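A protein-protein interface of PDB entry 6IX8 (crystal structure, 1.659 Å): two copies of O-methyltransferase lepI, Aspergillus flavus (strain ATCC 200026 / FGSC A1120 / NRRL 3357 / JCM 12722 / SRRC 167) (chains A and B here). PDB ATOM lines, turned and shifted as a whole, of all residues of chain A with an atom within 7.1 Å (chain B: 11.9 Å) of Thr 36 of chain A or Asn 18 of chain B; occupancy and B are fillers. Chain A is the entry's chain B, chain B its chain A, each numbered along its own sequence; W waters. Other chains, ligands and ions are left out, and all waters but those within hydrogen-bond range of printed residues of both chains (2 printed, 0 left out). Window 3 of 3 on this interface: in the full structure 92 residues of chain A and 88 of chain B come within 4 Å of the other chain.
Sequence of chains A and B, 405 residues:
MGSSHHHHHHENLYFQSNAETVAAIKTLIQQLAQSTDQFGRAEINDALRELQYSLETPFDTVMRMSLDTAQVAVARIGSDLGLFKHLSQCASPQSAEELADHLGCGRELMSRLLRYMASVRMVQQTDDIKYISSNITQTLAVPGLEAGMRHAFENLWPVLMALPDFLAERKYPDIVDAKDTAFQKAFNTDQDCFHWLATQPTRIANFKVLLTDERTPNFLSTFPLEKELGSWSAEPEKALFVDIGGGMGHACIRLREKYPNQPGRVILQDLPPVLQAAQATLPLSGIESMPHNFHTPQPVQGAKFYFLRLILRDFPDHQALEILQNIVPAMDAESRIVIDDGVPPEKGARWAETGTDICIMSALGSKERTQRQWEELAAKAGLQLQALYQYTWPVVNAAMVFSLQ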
ATOM      1  N   GLN A  31      15.252  -8.809 -32.860  1.00  0.00           N
ATOM      2  CA  GLN A  31      15.061  -9.602 -31.668  1.00  0.00           C
ATOM      3  C   GLN A  31      15.848  -9.036 -30.485  1.00  0.00           C
ATOM      4  O   GLN A  31      15.324  -8.961 -29.364  1.00  0.00           O
ATOM      5  CB  GLN A  31      15.478 -11.053 -31.971  1.00  0.00           C
ATOM      6  CG  GLN A  31      15.415 -11.968 -30.774  1.00  0.00           C
ATOM      7  CD  GLN A  31      14.004 -12.335 -30.363  1.00  0.00           C
ATOM      8  OE1 GLN A  31      13.023 -12.077 -31.093  1.00  0.00           O
ATOM      9  NE2 GLN A  31      13.893 -12.974 -29.185  1.00  0.00           N
ATOM     10  N   LEU A  32      17.094  -8.617 -30.723  1.00  0.00           N
ATOM     11  CA  LEU A  32      17.868  -7.992 -29.653  1.00  0.00           C
ATOM     12  C   LEU A  32      17.222  -6.681 -29.204  1.00  0.00           C
ATOM     13  O   LEU A  32      17.153  -6.389 -28.001  1.00  0.00           O
ATOM     14  CB  LEU A  32      19.281  -7.733 -30.128  1.00  0.00           C
ATOM     15  CG  LEU A  32      20.106  -9.002 -30.349  1.00  0.00           C
ATOM     16  CD1 LEU A  32      21.430  -8.663 -31.039  1.00  0.00           C
ATOM     17  CD2 LEU A  32      20.294  -9.751 -29.052  1.00  0.00           C
ATOM     18  N   ALA A  33      16.734  -5.898 -30.158  1.00  0.00           N
ATOM     19  CA  ALA A  33      16.081  -4.636 -29.779  1.00  0.00           C
ATOM     20  C   ALA A  33      14.845  -4.877 -28.908  1.00  0.00           C
ATOM     21  O   ALA A  33      14.622  -4.147 -27.931  1.00  0.00           O
ATOM     22  CB  ALA A  33      15.688  -3.843 -31.038  1.00  0.00           C
ATOM     23  N   GLN A  34      13.999  -5.846 -29.287  1.00  0.00           N
ATOM     24  CA  GLN A  34      12.739  -6.075 -28.558  1.00  0.00           C
ATOM     25  C   GLN A  34      12.970  -6.467 -27.129  1.00  0.00           C
ATOM     26  O   GLN A  34      12.116  -6.229 -26.263  1.00  0.00           O
ATOM     27  CB  GLN A  34      11.929  -7.209 -29.163  1.00  0.00           C
ATOM     28  CG  GLN A  34      11.156  -6.909 -30.381  1.00  0.00           C
ATOM     29  CD  GLN A  34      10.713  -8.207 -31.036  1.00  0.00           C
ATOM     30  OE1 GLN A  34      10.379  -9.180 -30.333  1.00  0.00           O
ATOM     31  NE2 GLN A  34      10.763  -8.255 -32.382  1.00  0.00           N
ATOM     32  N   SER A  35      14.083  -7.076 -26.862  1.00  0.00           N
ATOM     33  CA  SER A  35      14.297  -7.646 -25.561  1.00  0.00           C
ATOM     34  C   SER A  35      14.977  -6.688 -24.597  1.00  0.00           C
ATOM     35  O   SER A  35      15.085  -7.010 -23.416  1.00  0.00           O
ATOM     36  CB  SER A  35      15.091  -8.944 -25.742  1.00  0.00           C
ATOM     37  OG  SER A  35      14.453  -9.734 -26.753  1.00  0.00           O
ATOM     38  N   THR A  36      15.380  -5.509 -25.052  1.00  0.00           N
ATOM     39  CA  THR A  36      16.007  -4.558 -24.144  1.00  0.00           C
ATOM     40  C   THR A  36      14.963  -3.489 -23.862  1.00  0.00           C
ATOM     41  O   THR A  36      13.791  -3.661 -24.179  1.00  0.00           O
ATOM     42  CB  THR A  36      17.324  -4.026 -24.716  1.00  0.00           C
ATOM     43  OG1 THR A  36      17.994  -3.267 -23.705  1.00  0.00           O
ATOM     44  CG2 THR A  36      17.097  -3.204 -26.038  1.00  0.00           C
ATOM     45  N   ASP A  37      15.360  -2.431 -23.161  1.00  0.00           N
ATOM     46  CA  ASP A  37      14.447  -1.351 -22.841  1.00  0.00           C
ATOM     47  C   ASP A  37      14.768  -0.142 -23.722  1.00  0.00           C
ATOM     48  O   ASP A  37      15.581  -0.240 -24.648  1.00  0.00           O
ATOM     49  CB  ASP A  37      14.526  -1.024 -21.352  1.00  0.00           C
ATOM     50  CG  ASP A  37      15.869  -0.442 -20.954  1.00  0.00           C
ATOM     51  OD1 ASP A  37      16.762  -0.271 -21.814  1.00  0.00           O
ATOM     52  OD2 ASP A  37      16.044  -0.160 -19.750  1.00  0.00           O
ATOM     53  N   GLN A  38      14.063   0.971 -23.480  1.00  0.00           N
ATOM     54  CA  GLN A  38      14.164   2.097 -24.404  1.00  0.00           C
ATOM     55  C   GLN A  38      15.605   2.596 -24.494  1.00  0.00           C
ATOM     56  O   GLN A  38      16.051   3.034 -25.575  1.00  0.00           O
ATOM     57  CB  GLN A  38      13.198   3.226 -23.993  1.00  0.00           C
ATOM     58  CG  GLN A  38      13.442   3.850 -22.694  1.00  0.00           C
ATOM     59  CD  GLN A  38      12.468   5.024 -22.517  1.00  0.00           C
ATOM     60  OE1 GLN A  38      12.349   5.875 -23.423  1.00  0.00           O
ATOM     61  NE2 GLN A  38      11.743   5.037 -21.407  1.00  0.00           N
ATOM     62  N   PHE A  39      16.329   2.568 -23.369  1.00  0.00           N
ATOM     63  CA  PHE A  39      17.706   3.058 -23.342  1.00  0.00           C
ATOM     64  C   PHE A  39      18.624   2.129 -24.129  1.00  0.00           C
ATOM     65  O   PHE A  39      19.482   2.594 -24.891  1.00  0.00           O
ATOM     66  CB  PHE A  39      18.171   3.224 -21.896  1.00  0.00           C
ATOM     67  CG  PHE A  39      17.194   4.018 -21.063  1.00  0.00           C
ATOM     68  CD1 PHE A  39      16.777   5.274 -21.485  1.00  0.00           C
ATOM     69  CD2 PHE A  39      16.664   3.492 -19.893  1.00  0.00           C
ATOM     70  CE1 PHE A  39      15.852   6.037 -20.703  1.00  0.00           C
ATOM     71  CE2 PHE A  39      15.738   4.244 -19.127  1.00  0.00           C
ATOM     72  CZ  PHE A  39      15.351   5.497 -19.543  1.00  0.00           C
ATOM     73  N   GLY A  40      18.413   0.813 -24.000  1.00  0.00           N
ATOM     74  CA  GLY A  40      19.186  -0.118 -24.804  1.00  0.00           C
ATOM     75  C   GLY A  40      18.882   0.021 -26.290  1.00  0.00           C
ATOM     76  O   GLY A  40      19.768  -0.155 -27.122  1.00  0.00           O
ATOM     77  N   ARG A  41      17.626   0.276 -26.641  1.00  0.00           N
ATOM     78  CA  ARG A  41      17.302   0.447 -28.052  1.00  0.00           C
ATOM     79  C   ARG A  41      17.980   1.707 -28.589  1.00  0.00           C
ATOM     80  O   ARG A  41      18.431   1.733 -29.748  1.00  0.00           O
ATOM     81  CB  ARG A  41      15.794   0.534 -28.264  1.00  0.00           C
ATOM     82  CG  ARG A  41      15.139  -0.886 -28.432  1.00  0.00           C
ATOM     83  CD  ARG A  41      13.625  -0.796 -28.783  1.00  0.00           C
ATOM     84  NE  ARG A  41      12.876  -0.299 -27.639  1.00  0.00           N
ATOM     85  CZ  ARG A  41      12.573  -1.003 -26.554  1.00  0.00           C
ATOM     86  NH1 ARG A  41      11.879  -0.411 -25.550  1.00  0.00           N
ATOM     87  NH2 ARG A  41      12.923  -2.310 -26.465  1.00  0.00           N
ATOM     88  N   ALA A  42      18.044   2.752 -27.766  1.00  0.00           N
ATOM     89  CA  ALA A  42      18.717   3.985 -28.220  1.00  0.00           C
ATOM     90  C   ALA A  42      20.194   3.727 -28.453  1.00  0.00           C
ATOM     91  O   ALA A  42      20.781   4.248 -29.409  1.00  0.00           O
ATOM     92  CB  ALA A  42      18.543   5.113 -27.189  1.00  0.00           C
ATOM     93  N   GLU A  43      20.804   2.905 -27.601  1.00  0.00           N
ATOM     94  CA  GLU A  43      22.203   2.532 -27.809  1.00  0.00           C
ATOM     95  C   GLU A  43      22.373   1.679 -29.054  1.00  0.00           C
ATOM     96  O   GLU A  43      23.346   1.867 -29.814  1.00  0.00           O
ATOM     97  CB  GLU A  43      22.728   1.750 -26.604  1.00  0.00           C
ATOM     98  CG  GLU A  43      22.944   2.572 -25.368  1.00  0.00           C
ATOM     99  CD  GLU A  43      23.548   1.669 -24.304  1.00  0.00           C
ATOM    100  OE1 GLU A  43      24.801   1.464 -24.315  1.00  0.00           O
ATOM    101  OE2 GLU A  43      22.754   1.081 -23.530  1.00  0.00           O
ATOM    102  N   ILE A  44      21.441   0.747 -29.308  1.00  0.00           N
ATOM    103  CA  ILE A  44      21.528  -0.018 -30.564  1.00  0.00           C
ATOM    104  C   ILE A  44      21.394   0.910 -31.760  1.00  0.00           C
ATOM    105  O   ILE A  44      22.133   0.790 -32.744  1.00  0.00           O
ATOM    106  CB  ILE A  44      20.462  -1.113 -30.612  1.00  0.00           C
ATOM    107  CG1 ILE A  44      20.826  -2.189 -29.592  1.00  0.00           C
ATOM    108  CG2 ILE A  44      20.343  -1.792 -32.064  1.00  0.00           C
ATOM    109  CD1 ILE A  44      19.765  -3.256 -29.504  1.00  0.00           C
ATOM    110  N   SER B  17      25.361  -7.446 -20.501  1.00  0.00           N
ATOM    111  CA  SER B  17      25.832  -6.055 -20.553  1.00  0.00           C
ATOM    112  C   SER B  17      25.406  -5.323 -21.838  1.00  0.00           C
ATOM    113  O   SER B  17      25.710  -5.780 -22.958  1.00  0.00           O
ATOM    114  CB  SER B  17      27.364  -5.999 -20.432  1.00  0.00           C
ATOM    115  OG  SER B  17      27.860  -4.763 -20.941  1.00  0.00           O
ATOM    116  N   ASN B  18      24.723  -4.183 -21.680  1.00  0.00           N
ATOM    117  CA  ASN B  18      24.241  -3.439 -22.847  1.00  0.00           C
ATOM    118  C   ASN B  18      25.376  -3.076 -23.779  1.00  0.00           C
ATOM    119  O   ASN B  18      25.311  -3.309 -25.001  1.00  0.00           O
ATOM    120  CB  ASN B  18      23.549  -2.172 -22.404  1.00  0.00           C
ATOM    121  CG  ASN B  18      22.090  -2.309 -22.473  1.00  0.00           C
ATOM    122  OD1 ASN B  18      21.585  -3.426 -22.455  1.00  0.00           O
ATOM    123  ND2 ASN B  18      21.380  -1.184 -22.557  1.00  0.00           N
ATOM    124  N   ALA B  19      26.424  -2.502 -23.205  1.00  0.00           N
ATOM    125  CA  ALA B  19      27.614  -2.135 -23.944  1.00  0.00           C
ATOM    126  C   ALA B  19      28.209  -3.346 -24.639  1.00  0.00           C
ATOM    127  O   ALA B  19      28.701  -3.231 -25.755  1.00  0.00           O
ATOM    128  CB  ALA B  19      28.643  -1.529 -22.999  1.00  0.00           C
ATOM    129  N   GLU B  20      28.222  -4.484 -23.952  1.00  0.00           N
ATOM    130  CA  GLU B  20      28.830  -5.682 -24.522  1.00  0.00           C
ATOM    131  C   GLU B  20      28.042  -6.156 -25.739  1.00  0.00           C
ATOM    132  O   GLU B  20      28.630  -6.577 -26.736  1.00  0.00           O
ATOM    133  CB  GLU B  20      28.925  -6.775 -23.450  1.00  0.00           C
ATOM    134  CG  GLU B  20      29.734  -7.989 -23.848  1.00  0.00           C
ATOM    135  CD  GLU B  20      29.660  -9.098 -22.797  1.00  0.00           C
ATOM    136  OE1 GLU B  20      29.668  -8.725 -21.589  1.00  0.00           O
ATOM    137  OE2 GLU B  20      29.567 -10.313 -23.182  1.00  0.00           O
ATOM    138  N   THR B  21      26.706  -6.133 -25.654  1.00  0.00           N
ATOM    139  CA  THR B  21      25.874  -6.539 -26.785  1.00  0.00           C
ATOM    140  C   THR B  21      26.068  -5.602 -27.986  1.00  0.00           C
ATOM    141  O   THR B  21      26.231  -6.073 -29.117  1.00  0.00           O
ATOM    142  CB  THR B  21      24.397  -6.604 -26.353  1.00  0.00           C
ATOM    143  OG1 THR B  21      24.255  -7.607 -25.354  1.00  0.00           O
ATOM    144  CG2 THR B  21      23.503  -7.068 -27.539  1.00  0.00           C
ATOM    145  N   VAL B  22      26.110  -4.285 -27.754  1.00  0.00           N
ATOM    146  CA  VAL B  22      26.336  -3.339 -28.860  1.00  0.00           C
ATOM    147  C   VAL B  22      27.713  -3.557 -29.480  1.00  0.00           C
ATOM    148  O   VAL B  22      27.872  -3.565 -30.712  1.00  0.00           O
ATOM    149  CB  VAL B  22      26.161  -1.900 -28.332  1.00  0.00           C
ATOM    150  CG1 VAL B  22      26.855  -0.846 -29.212  1.00  0.00           C
ATOM    151  CG2 VAL B  22      24.690  -1.637 -28.157  1.00  0.00           C
ATOM    152  N   ALA B  23      28.730  -3.779 -28.657  1.00  0.00           N
ATOM    153  CA  ALA B  23      30.044  -3.986 -29.254  1.00  0.00           C
ATOM    154  C   ALA B  23      30.085  -5.294 -30.072  1.00  0.00           C
ATOM    155  O   ALA B  23      30.756  -5.372 -31.105  1.00  0.00           O
ATOM    156  CB  ALA B  23      31.112  -4.015 -28.138  1.00  0.00           C
ATOM    157  N   ALA B  24      29.356  -6.319 -29.627  1.00  0.00           N
ATOM    158  CA  ALA B  24      29.300  -7.564 -30.386  1.00  0.00           C
ATOM    159  C   ALA B  24      28.533  -7.393 -31.694  1.00  0.00           C
ATOM    160  O   ALA B  24      28.914  -7.965 -32.708  1.00  0.00           O
ATOM    161  CB  ALA B  24      28.681  -8.695 -29.546  1.00  0.00           C
ATOM    162  N   ILE B  25      27.430  -6.622 -31.686  1.00  0.00           N
ATOM    163  CA  ILE B  25      26.777  -6.293 -32.962  1.00  0.00           C
ATOM    164  C   ILE B  25      27.770  -5.614 -33.923  1.00  0.00           C
ATOM    165  O   ILE B  25      27.856  -5.971 -35.099  1.00  0.00           O
ATOM    166  CB  ILE B  25      25.551  -5.383 -32.708  1.00  0.00           C
ATOM    167  CG1 ILE B  25      24.447  -6.139 -31.975  1.00  0.00           C
ATOM    168  CG2 ILE B  25      25.126  -4.775 -34.023  1.00  0.00           C
ATOM    169  CD1 ILE B  25      23.382  -5.107 -31.378  1.00  0.00           C
ATOM    170  N   LYS B  26      28.540  -4.636 -33.429  1.00  0.00           N
ATOM    171  CA  LYS B  26      29.507  -3.962 -34.295  1.00  0.00           C
ATOM    172  C   LYS B  26      30.525  -4.940 -34.844  1.00  0.00           C
ATOM    173  O   LYS B  26      30.818  -4.942 -36.038  1.00  0.00           O
ATOM    174  CB  LYS B  26      30.220  -2.818 -33.526  1.00  0.00           C
ATOM    175  CG  LYS B  26      29.259  -1.684 -33.248  1.00  0.00           C
ATOM    176  CD  LYS B  26      30.035  -0.501 -32.693  1.00  0.00           C
ATOM    177  CE  LYS B  26      29.126   0.387 -31.878  1.00  0.00           C
ATOM    178  NZ  LYS B  26      29.911   1.538 -31.292  1.00  0.00           N
ATOM    179  N   THR B  27      31.053  -5.821 -33.988  1.00  0.00           N
ATOM    180  CA  THR B  27      32.040  -6.773 -34.461  1.00  0.00           C
ATOM    181  C   THR B  27      31.461  -7.680 -35.534  1.00  0.00           C
ATOM    182  O   THR B  27      32.092  -7.916 -36.563  1.00  0.00           O
ATOM    183  CB  THR B  27      32.575  -7.616 -33.271  1.00  0.00           C
ATOM    184  OG1 THR B  27      33.269  -6.764 -32.351  1.00  0.00           O
ATOM    185  CG2 THR B  27      33.523  -8.729 -33.749  1.00  0.00           C
ATOM    186  N   LEU B  55      13.356   1.199 -35.814  1.00  0.00           N
ATOM    187  CA  LEU B  55      13.510   1.120 -34.373  1.00  0.00           C
ATOM    188  C   LEU B  55      13.527   2.465 -33.658  1.00  0.00           C
ATOM    189  O   LEU B  55      13.497   2.505 -32.428  1.00  0.00           O
ATOM    190  CB  LEU B  55      14.783   0.354 -34.036  1.00  0.00           C
ATOM    191  CG  LEU B  55      14.664  -1.069 -34.569  1.00  0.00           C
ATOM    192  CD1 LEU B  55      16.047  -1.756 -34.580  1.00  0.00           C
ATOM    193  CD2 LEU B  55      13.608  -1.917 -33.798  1.00  0.00           C
ATOM    194  N   GLU B  56      13.559   3.585 -34.375  1.00  0.00           N
ATOM    195  CA  GLU B  56      13.606   4.862 -33.690  1.00  0.00           C
ATOM    196  C   GLU B  56      12.235   5.179 -33.106  1.00  0.00           C
ATOM    197  O   GLU B  56      11.212   4.704 -33.588  1.00  0.00           O
ATOM    198  CB  GLU B  56      14.035   5.980 -34.660  1.00  0.00           C
ATOM    199  CG  GLU B  56      13.055   6.155 -35.762  1.00  0.00           C
ATOM    200  CD  GLU B  56      13.535   7.112 -36.908  1.00  0.00           C
ATOM    201  OE1 GLU B  56      14.699   7.495 -36.929  1.00  0.00           O
ATOM    202  OE2 GLU B  56      12.729   7.449 -37.768  1.00  0.00           O
ATOM    203  N   THR B  57      12.243   5.949 -32.024  1.00  0.00           N
ATOM    204  CA  THR B  57      10.972   6.406 -31.432  1.00  0.00           C
ATOM    205  C   THR B  57      10.417   7.561 -32.254  1.00  0.00           C
ATOM    206  O   THR B  57      11.125   8.166 -33.059  1.00  0.00           O
ATOM    207  CB  THR B  57      11.177   6.906 -30.007  1.00  0.00           C
ATOM    208  OG1 THR B  57      12.034   8.067 -30.006  1.00  0.00           O
ATOM    209  CG2 THR B  57      11.795   5.810 -29.111  1.00  0.00           C
ATOM    210  N   ASP B  60      12.615  10.436 -31.759  1.00  0.00           N
ATOM    211  CA  ASP B  60      13.856  10.198 -32.501  1.00  0.00           C
ATOM    212  C   ASP B  60      13.729  10.606 -33.953  1.00  0.00           C
ATOM    213  O   ASP B  60      14.678  11.109 -34.547  1.00  0.00           O
ATOM    214  CB  ASP B  60      14.190   8.694 -32.521  1.00  0.00           C
ATOM    215  CG  ASP B  60      14.788   8.167 -31.234  1.00  0.00           C
ATOM    216  OD1 ASP B  60      15.202   8.983 -30.392  1.00  0.00           O
ATOM    217  OD2 ASP B  60      14.808   6.882 -31.093  1.00  0.00           O
HETATM  218  O   HOH W   1      15.742   3.932 -30.128  1.00  0.00           O
HETATM  219  O   HOH W   2      19.067  -0.848 -21.225  1.00  0.00           O
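Water W2 lies within hydrogen-bond range of OD1 of Asp 37 of chain A (2.4 Å), ND2 of Asn 18 of chain B (2.7 Å) and N of Gly 40 of chain A (3.3 Å).
Water W1 bridges the side-chain carboxylate (OD2) of Asp 60 of chain B and the backbone carbonyl oxygen (O) of Arg 41 of chain A.
Among the printed residues, merely in contact across the chains: Ala 33 of chain A with Leu 55 of chain B, Thr 36 of chain A with Asn 18 of chain B and Gly 40 of chain A with Asn 18 of chain B.
No position is printed for both chains.
Of the 4 pairs that touch across the chains among the printed residues, none has its exchanged pair printed and touching as well.
O of Ala 33 of chain A sits at hydrogen-bond distance from NH2 of Arg 41 of chain A, 2.9 Å away.
The guanidinium group of Arg 41 of chain A lies within hydrogen-bond range of the backbone carbonyl oxygen of Thr 36 of chain A, at 2.8 Å.
N of Gly 40 of chain A is in hydrogen-bond range of OD1 of Asp 37 of chain A (2.9 Å).
Leu 32 of chain A touches none of the printed residues of chain B.
Of chain B, only Leu 55 comes within 4 Å of Ala 33 of chain A.
Gln 34 of chain A touches none of the printed residues of chain B.
Thr 36 of chain A touches just one residue of chain B: Asn 18.
No residue of chain B comes within 4 Å of Asp 37 of chain A.
Gly 40 of chain A touches just one residue of chain B: Asn 18 (3.3 Å).
Glu 43 of chain A touches just one residue of chain B: Asn 18.
Of the printed residues of chain A, Asn 18 of chain B touches Thr 36 (3.8 Å), Gly 40 (3.3 Å) and Glu 43 (2.8 Å).
Printed residues of chain A within 4 Å of Leu 55 of chain B: Ala 33.
The nearest printed residue of chain A that does not touch Leu 55 of chain B is Arg 41 of chain A (4.9 Å).
The side-chain amide nitrogen of Asn 18 of chain B sits at hydrogen-bond distance from the side-chain carboxylate of Glu 43 of chain A, at 2.8 Å.
Of the 15 printed residues of chain B, 2 touch a printed residue of chain A.
Of the 14 printed residues of chain A, 4 touch a printed residue of chain B.
Hydrophobic or aromatic side chains of chain A that line the printed part of chain B: Ala 33.
Among the printed residues, no Asp or Glu carboxylate lies within 4 Å of a Lys or Arg side-chain nitrogen of the other chain.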
